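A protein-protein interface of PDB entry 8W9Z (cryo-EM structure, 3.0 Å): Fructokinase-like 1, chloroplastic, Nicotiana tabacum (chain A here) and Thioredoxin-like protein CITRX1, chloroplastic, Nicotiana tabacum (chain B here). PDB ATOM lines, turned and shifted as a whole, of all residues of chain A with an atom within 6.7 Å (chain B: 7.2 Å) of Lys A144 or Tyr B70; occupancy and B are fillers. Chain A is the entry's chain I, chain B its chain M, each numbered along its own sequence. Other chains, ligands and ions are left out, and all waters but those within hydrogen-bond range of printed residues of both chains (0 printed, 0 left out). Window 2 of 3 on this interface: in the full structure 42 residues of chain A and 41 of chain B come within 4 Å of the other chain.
Among the printed residues, pairs that only touch across the chains: Asp A143 with Tyr B70, Lys A144 with Tyr B70, His A141 with Thr B99, Tyr A145 with Glu B112, Met A140 with Thr B99 and Trp A148 with Thr B99.
Of the printed residues of chain B, Met A140 touches Thr B99 (3.8 Å).
Of the printed residues of chain B, Asp A143 touches Tyr B70 (3.3 Å) and Lys B126 (3.1 Å).
Lys A144 touches just one residue of chain B: Tyr B70.
Printed residues of chain B within 4 Å of Tyr A145: Glu B112.
Glu A147 touches none of the printed residues of chain B.
Tyr B70 touches two residues of chain A.
Leu B71 touches none of the printed residues of chain A.
Of the printed residues of chain A, Thr B99 touches Met A140 (3.8 Å), His A141 (3.7 Å) and Trp A148 (3.9 Å).
The nearest residue of chain B that does not touch Lys A144 is Lys B126 (6.1 Å).
The nearest residue of chain A that does not touch Tyr B70 is Tyr A145 (4.1 Å).
The nearest printed residue of chain B that does not touch Gln A142 is Thr B99 (5.5 Å).
ND1 of His A141 sits at hydrogen-bond distance from N of Asp A143, at 3.2 Å.
O of Lys B73 sits at hydrogen-bond distance from N of Lys B126, 3.2 Å away.
N of His A141 sits close to OE2 of Glu A147.
A ring nitrogen (ND1) of His A141 lies within hydrogen-bond range of the backbone NH (N) of Lys A144 (3.4 Å).
NE1 of Trp A148 lies within hydrogen-bond range of O of His A141 (2.9 Å).
O of Lys A144 is in hydrogen-bond range of NE1 of Trp A148, at 3.2 Å.
Of the 10 printed residues of chain B, 4 touch a printed residue of chain A.
Printed residues of chain B that touch a printed residue of chain A: Tyr B70, Thr B99, Glu B112 and Lys B126.
Hydrophobic or aromatic side chains of chain B that line the printed part of chain A: Tyr B70.
Along chain B the printed residues that touch a printed residue of chain A span positions 70 to 126.
Printed residues of chain A that touch a printed residue of chain B: Met A140, His A141, Gln A142, Asp A143, Lys A144, Tyr A145 and Trp A148.
Hydrophobic or aromatic side chains of chain A that line the printed part of chain B: Tyr A145 and Trp A148.
Among the printed residues, 8 pairs touch across the chains.
The backbone carbonyl oxygen (O) of Gln A142 is in hydrogen-bond range of the side-chain amino group (NZ) of Lys B126.
OD1 of Asp A143 is in salt-bridge range of NZ of Lys B126 (3.1 Å).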
ATOM      1  N   MET A 140       2.431  -1.395  13.824  1.00  0.00           N
ATOM      2  CA  MET A 140       2.071  -0.933  12.491  1.00  0.00           C
ATOM      3  C   MET A 140       2.951  -1.622  11.448  1.00  0.00           C
ATOM      4  O   MET A 140       3.705  -2.550  11.754  1.00  0.00           O
ATOM      5  CB  MET A 140       2.178   0.591  12.404  1.00  0.00           C
ATOM      6  CG  MET A 140       0.982   1.328  12.975  1.00  0.00           C
ATOM      7  SD  MET A 140      -0.534   0.968  12.069  1.00  0.00           S
ATOM      8  CE  MET A 140      -1.722   1.956  12.973  1.00  0.00           C
ATOM      9  N   HIS A 141       2.837  -1.161  10.205  1.00  0.00           N
ATOM     10  CA  HIS A 141       3.559  -1.767   9.096  1.00  0.00           C
ATOM     11  C   HIS A 141       5.067  -1.635   9.294  1.00  0.00           C
ATOM     12  O   HIS A 141       5.556  -0.775  10.032  1.00  0.00           O
ATOM     13  CB  HIS A 141       3.143  -1.122   7.776  1.00  0.00           C
ATOM     14  CG  HIS A 141       3.389  -1.982   6.575  1.00  0.00           C
ATOM     15  ND1 HIS A 141       4.553  -1.918   5.840  1.00  0.00           N
ATOM     16  CD2 HIS A 141       2.618  -2.920   5.979  1.00  0.00           C
ATOM     17  CE1 HIS A 141       4.489  -2.783   4.843  1.00  0.00           C
ATOM     18  NE2 HIS A 141       3.325  -3.404   4.905  1.00  0.00           N
ATOM     19  N   GLN A 142       5.809  -2.508   8.612  1.00  0.00           N
ATOM     20  CA  GLN A 142       7.259  -2.541   8.763  1.00  0.00           C
ATOM     21  C   GLN A 142       7.929  -1.406   8.000  1.00  0.00           C
ATOM     22  O   GLN A 142       8.792  -0.707   8.544  1.00  0.00           O
ATOM     23  CB  GLN A 142       7.804  -3.886   8.281  1.00  0.00           C
ATOM     24  CG  GLN A 142       7.125  -5.095   8.889  1.00  0.00           C
ATOM     25  CD  GLN A 142       7.632  -6.394   8.298  1.00  0.00           C
ATOM     26  OE1 GLN A 142       7.198  -7.479   8.687  1.00  0.00           O
ATOM     27  NE2 GLN A 142       8.557  -6.289   7.350  1.00  0.00           N
ATOM     28  N   ASP A 143       7.547  -1.210   6.740  1.00  0.00           N
ATOM     29  CA  ASP A 143       8.241  -0.289   5.849  1.00  0.00           C
ATOM     30  C   ASP A 143       7.523   1.040   5.671  1.00  0.00           C
ATOM     31  O   ASP A 143       8.175   2.087   5.622  1.00  0.00           O
ATOM     32  CB  ASP A 143       8.440  -0.942   4.478  1.00  0.00           C
ATOM     33  CG  ASP A 143       9.181  -2.260   4.563  1.00  0.00           C
ATOM     34  OD1 ASP A 143      10.010  -2.419   5.482  1.00  0.00           O
ATOM     35  OD2 ASP A 143       8.933  -3.138   3.710  1.00  0.00           O
ATOM     36  N   LYS A 144       6.194   1.029   5.574  1.00  0.00           N
ATOM     37  CA  LYS A 144       5.448   2.251   5.303  1.00  0.00           C
ATOM     38  C   LYS A 144       5.427   3.167   6.518  1.00  0.00           C
ATOM     39  O   LYS A 144       4.581   3.013   7.404  1.00  0.00           O
ATOM     40  CB  LYS A 144       4.019   1.921   4.868  1.00  0.00           C
ATOM     41  CG  LYS A 144       3.931   1.084   3.605  1.00  0.00           C
ATOM     42  CD  LYS A 144       2.487   0.819   3.219  1.00  0.00           C
ATOM     43  CE  LYS A 144       2.398  -0.024   1.958  1.00  0.00           C
ATOM     44  NZ  LYS A 144       0.987  -0.291   1.567  1.00  0.00           N
ATOM     45  N   TYR A 145       6.354   4.124   6.569  1.00  0.00           N
ATOM     46  CA  TYR A 145       6.367   5.105   7.645  1.00  0.00           C
ATOM     47  C   TYR A 145       5.305   6.182   7.472  1.00  0.00           C
ATOM     48  O   TYR A 145       5.125   7.002   8.379  1.00  0.00           O
ATOM     49  CB  TYR A 145       7.749   5.756   7.757  1.00  0.00           C
ATOM     50  CG  TYR A 145       8.334   6.217   6.442  1.00  0.00           C
ATOM     51  CD1 TYR A 145       7.967   7.431   5.881  1.00  0.00           C
ATOM     52  CD2 TYR A 145       9.264   5.438   5.768  1.00  0.00           C
ATOM     53  CE1 TYR A 145       8.503   7.853   4.681  1.00  0.00           C
ATOM     54  CE2 TYR A 145       9.805   5.853   4.568  1.00  0.00           C
ATOM     55  CZ  TYR A 145       9.422   7.062   4.029  1.00  0.00           C
ATOM     56  OH  TYR A 145       9.960   7.476   2.834  1.00  0.00           O
ATOM     57  N   SER A 146       4.603   6.202   6.337  1.00  0.00           N
ATOM     58  CA  SER A 146       3.530   7.169   6.139  1.00  0.00           C
ATOM     59  C   SER A 146       2.325   6.882   7.022  1.00  0.00           C
ATOM     60  O   SER A 146       1.499   7.777   7.229  1.00  0.00           O
ATOM     61  CB  SER A 146       3.106   7.190   4.671  1.00  0.00           C
ATOM     62  OG  SER A 146       2.642   5.918   4.256  1.00  0.00           O
ATOM     63  N   GLU A 147       2.202   5.662   7.540  1.00  0.00           N
ATOM     64  CA  GLU A 147       1.107   5.299   8.427  1.00  0.00           C
ATOM     65  C   GLU A 147       1.558   5.117   9.871  1.00  0.00           C
ATOM     66  O   GLU A 147       0.758   4.694  10.709  1.00  0.00           O
ATOM     67  CB  GLU A 147       0.416   4.030   7.925  1.00  0.00           C
ATOM     68  CG  GLU A 147       1.243   2.767   8.052  1.00  0.00           C
ATOM     69  CD  GLU A 147       0.494   1.542   7.568  1.00  0.00           C
ATOM     70  OE1 GLU A 147      -0.095   1.602   6.469  1.00  0.00           O
ATOM     71  OE2 GLU A 147       0.482   0.525   8.292  1.00  0.00           O
ATOM     72  N   TRP A 148       2.818   5.428  10.179  1.00  0.00           N
ATOM     73  CA  TRP A 148       3.286   5.413  11.558  1.00  0.00           C
ATOM     74  C   TRP A 148       2.771   6.597  12.362  1.00  0.00           C
ATOM     75  O   TRP A 148       2.852   6.568  13.595  1.00  0.00           O
ATOM     76  CB  TRP A 148       4.815   5.402  11.604  1.00  0.00           C
ATOM     77  CG  TRP A 148       5.437   4.141  11.103  1.00  0.00           C
ATOM     78  CD1 TRP A 148       4.792   3.033  10.645  1.00  0.00           C
ATOM     79  CD2 TRP A 148       6.837   3.857  11.014  1.00  0.00           C
ATOM     80  NE1 TRP A 148       5.703   2.076  10.270  1.00  0.00           N
ATOM     81  CE2 TRP A 148       6.966   2.559  10.488  1.00  0.00           C
ATOM     82  CE3 TRP A 148       7.994   4.576  11.323  1.00  0.00           C
ATOM     83  CZ2 TRP A 148       8.205   1.963  10.267  1.00  0.00           C
ATOM     84  CZ3 TRP A 148       9.221   3.984  11.104  1.00  0.00           C
ATOM     85  CH2 TRP A 148       9.317   2.692  10.580  1.00  0.00           C
ATOM     86  N   ARG B  67       9.696  -2.579  -9.346  1.00  0.00           N
ATOM     87  CA  ARG B  67      10.793  -2.494  -8.392  1.00  0.00           C
ATOM     88  C   ARG B  67      10.240  -2.266  -6.992  1.00  0.00           C
ATOM     89  O   ARG B  67       9.236  -1.571  -6.815  1.00  0.00           O
ATOM     90  CB  ARG B  67      11.754  -1.365  -8.773  1.00  0.00           C
ATOM     91  CG  ARG B  67      13.005  -1.274  -7.914  1.00  0.00           C
ATOM     92  CD  ARG B  67      13.890  -2.495  -8.094  1.00  0.00           C
ATOM     93  NE  ARG B  67      15.131  -2.384  -7.333  1.00  0.00           N
ATOM     94  CZ  ARG B  67      16.073  -3.320  -7.300  1.00  0.00           C
ATOM     95  NH1 ARG B  67      15.917  -4.445  -7.986  1.00  0.00           N
ATOM     96  NH2 ARG B  67      17.171  -3.135  -6.580  1.00  0.00           N
ATOM     97  N   GLU B  68      10.899  -2.860  -6.001  1.00  0.00           N
ATOM     98  CA  GLU B  68      10.484  -2.686  -4.616  1.00  0.00           C
ATOM     99  C   GLU B  68      10.668  -1.237  -4.183  1.00  0.00           C
ATOM    100  O   GLU B  68      11.701  -0.617  -4.454  1.00  0.00           O
ATOM    101  CB  GLU B  68      11.280  -3.613  -3.698  1.00  0.00           C
ATOM    102  CG  GLU B  68      11.025  -5.099  -3.916  1.00  0.00           C
ATOM    103  CD  GLU B  68      11.764  -5.655  -5.119  1.00  0.00           C
ATOM    104  OE1 GLU B  68      12.614  -4.935  -5.684  1.00  0.00           O
ATOM    105  OE2 GLU B  68      11.494  -6.814  -5.499  1.00  0.00           O
ATOM    106  N   ASP B  69       9.654  -0.697  -3.507  1.00  0.00           N
ATOM    107  CA  ASP B  69       9.722   0.688  -3.052  1.00  0.00           C
ATOM    108  C   ASP B  69      10.746   0.849  -1.936  1.00  0.00           C
ATOM    109  O   ASP B  69      11.513   1.818  -1.918  1.00  0.00           O
ATOM    110  CB  ASP B  69       8.342   1.155  -2.587  1.00  0.00           C
ATOM    111  CG  ASP B  69       7.255   0.863  -3.601  1.00  0.00           C
ATOM    112  OD1 ASP B  69       7.575   0.750  -4.802  1.00  0.00           O
ATOM    113  OD2 ASP B  69       6.080   0.749  -3.195  1.00  0.00           O
ATOM    114  N   TYR B  70      10.772  -0.092  -0.998  1.00  0.00           N
ATOM    115  CA  TYR B  70      11.662  -0.036   0.152  1.00  0.00           C
ATOM    116  C   TYR B  70      12.793  -1.042  -0.015  1.00  0.00           C
ATOM    117  O   TYR B  70      12.590  -2.139  -0.544  1.00  0.00           O
ATOM    118  CB  TYR B  70      10.886  -0.313   1.440  1.00  0.00           C
ATOM    119  CG  TYR B  70       9.671   0.573   1.611  1.00  0.00           C
ATOM    120  CD1 TYR B  70       8.434   0.196   1.104  1.00  0.00           C
ATOM    121  CD2 TYR B  70       9.764   1.787   2.274  1.00  0.00           C
ATOM    122  CE1 TYR B  70       7.325   1.006   1.257  1.00  0.00           C
ATOM    123  CE2 TYR B  70       8.662   2.602   2.430  1.00  0.00           C
ATOM    124  CZ  TYR B  70       7.446   2.207   1.921  1.00  0.00           C
ATOM    125  OH  TYR B  70       6.347   3.020   2.078  1.00  0.00           O
ATOM    126  N   LEU B  71      13.990  -0.662   0.438  1.00  0.00           N
ATOM    127  CA  LEU B  71      15.183  -1.472   0.241  1.00  0.00           C
ATOM    128  C   LEU B  71      15.793  -2.020   1.521  1.00  0.00           C
ATOM    129  O   LEU B  71      16.579  -2.970   1.445  1.00  0.00           O
ATOM    130  CB  LEU B  71      16.263  -0.670  -0.506  1.00  0.00           C
ATOM    131  CG  LEU B  71      16.116  -0.483  -2.018  1.00  0.00           C
ATOM    132  CD1 LEU B  71      15.028   0.525  -2.363  1.00  0.00           C
ATOM    133  CD2 LEU B  71      17.444  -0.068  -2.633  1.00  0.00           C
ATOM    134  N   VAL B  72      15.464  -1.464   2.683  1.00  0.00           N
ATOM    135  CA  VAL B  72      16.005  -1.940   3.950  1.00  0.00           C
ATOM    136  C   VAL B  72      15.102  -3.052   4.469  1.00  0.00           C
ATOM    137  O   VAL B  72      13.932  -2.815   4.789  1.00  0.00           O
ATOM    138  CB  VAL B  72      16.122  -0.799   4.971  1.00  0.00           C
ATOM    139  CG1 VAL B  72      16.706  -1.315   6.273  1.00  0.00           C
ATOM    140  CG2 VAL B  72      16.974   0.324   4.411  1.00  0.00           C
ATOM    141  N   LYS B  73      15.646  -4.262   4.556  1.00  0.00           N
ATOM    142  CA  LYS B  73      14.878  -5.428   4.965  1.00  0.00           C
ATOM    143  C   LYS B  73      14.910  -5.593   6.478  1.00  0.00           C
ATOM    144  O   LYS B  73      15.853  -5.170   7.152  1.00  0.00           O
ATOM    145  CB  LYS B  73      15.418  -6.689   4.291  1.00  0.00           C
ATOM    146  CG  LYS B  73      15.410  -6.627   2.773  1.00  0.00           C
ATOM    147  CD  LYS B  73      14.011  -6.364   2.243  1.00  0.00           C
ATOM    148  CE  LYS B  73      14.005  -6.251   0.728  1.00  0.00           C
ATOM    149  NZ  LYS B  73      12.644  -5.951   0.202  1.00  0.00           N
ATOM    150  N   THR B  99       7.869   1.316  15.634  1.00  0.00           N
ATOM    151  CA  THR B  99       6.901   2.045  14.893  1.00  0.00           C
ATOM    152  C   THR B  99       6.391   3.231  15.672  1.00  0.00           C
ATOM    153  O   THR B  99       6.094   4.250  15.107  1.00  0.00           O
ATOM    154  CB  THR B  99       5.803   1.132  14.446  1.00  0.00           C
ATOM    155  OG1 THR B  99       5.211   0.518  15.588  1.00  0.00           O
ATOM    156  CG2 THR B  99       6.370   0.065  13.552  1.00  0.00           C
ATOM    157  N   GLU B 112      17.406   4.801   4.016  1.00  0.00           N
ATOM    158  CA  GLU B 112      17.112   4.422   2.637  1.00  0.00           C
ATOM    159  C   GLU B 112      18.020   5.153   1.656  1.00  0.00           C
ATOM    160  O   GLU B 112      18.496   4.557   0.681  1.00  0.00           O
ATOM    161  CB  GLU B 112      15.645   4.694   2.314  1.00  0.00           C
ATOM    162  CG  GLU B 112      14.691   3.689   2.921  1.00  0.00           C
ATOM    163  CD  GLU B 112      13.267   3.889   2.452  1.00  0.00           C
ATOM    164  OE1 GLU B 112      12.833   5.055   2.337  1.00  0.00           O
ATOM    165  OE2 GLU B 112      12.587   2.878   2.188  1.00  0.00           O
ATOM    166  N   LYS B 126      17.492  -3.669   9.444  1.00  0.00           N
ATOM    167  CA  LYS B 126      16.819  -3.056  10.580  1.00  0.00           C
ATOM    168  C   LYS B 126      16.119  -4.120  11.412  1.00  0.00           C
ATOM    169  O   LYS B 126      15.588  -5.096  10.874  1.00  0.00           O
ATOM    170  CB  LYS B 126      15.809  -1.996  10.126  1.00  0.00           C
ATOM    171  CG  LYS B 126      14.705  -2.520   9.227  1.00  0.00           C
ATOM    172  CD  LYS B 126      13.728  -1.418   8.857  1.00  0.00           C
ATOM    173  CE  LYS B 126      12.610  -1.944   7.976  1.00  0.00           C
ATOM    174  NZ  LYS B 126      11.654  -0.872   7.590  1.00  0.00           N
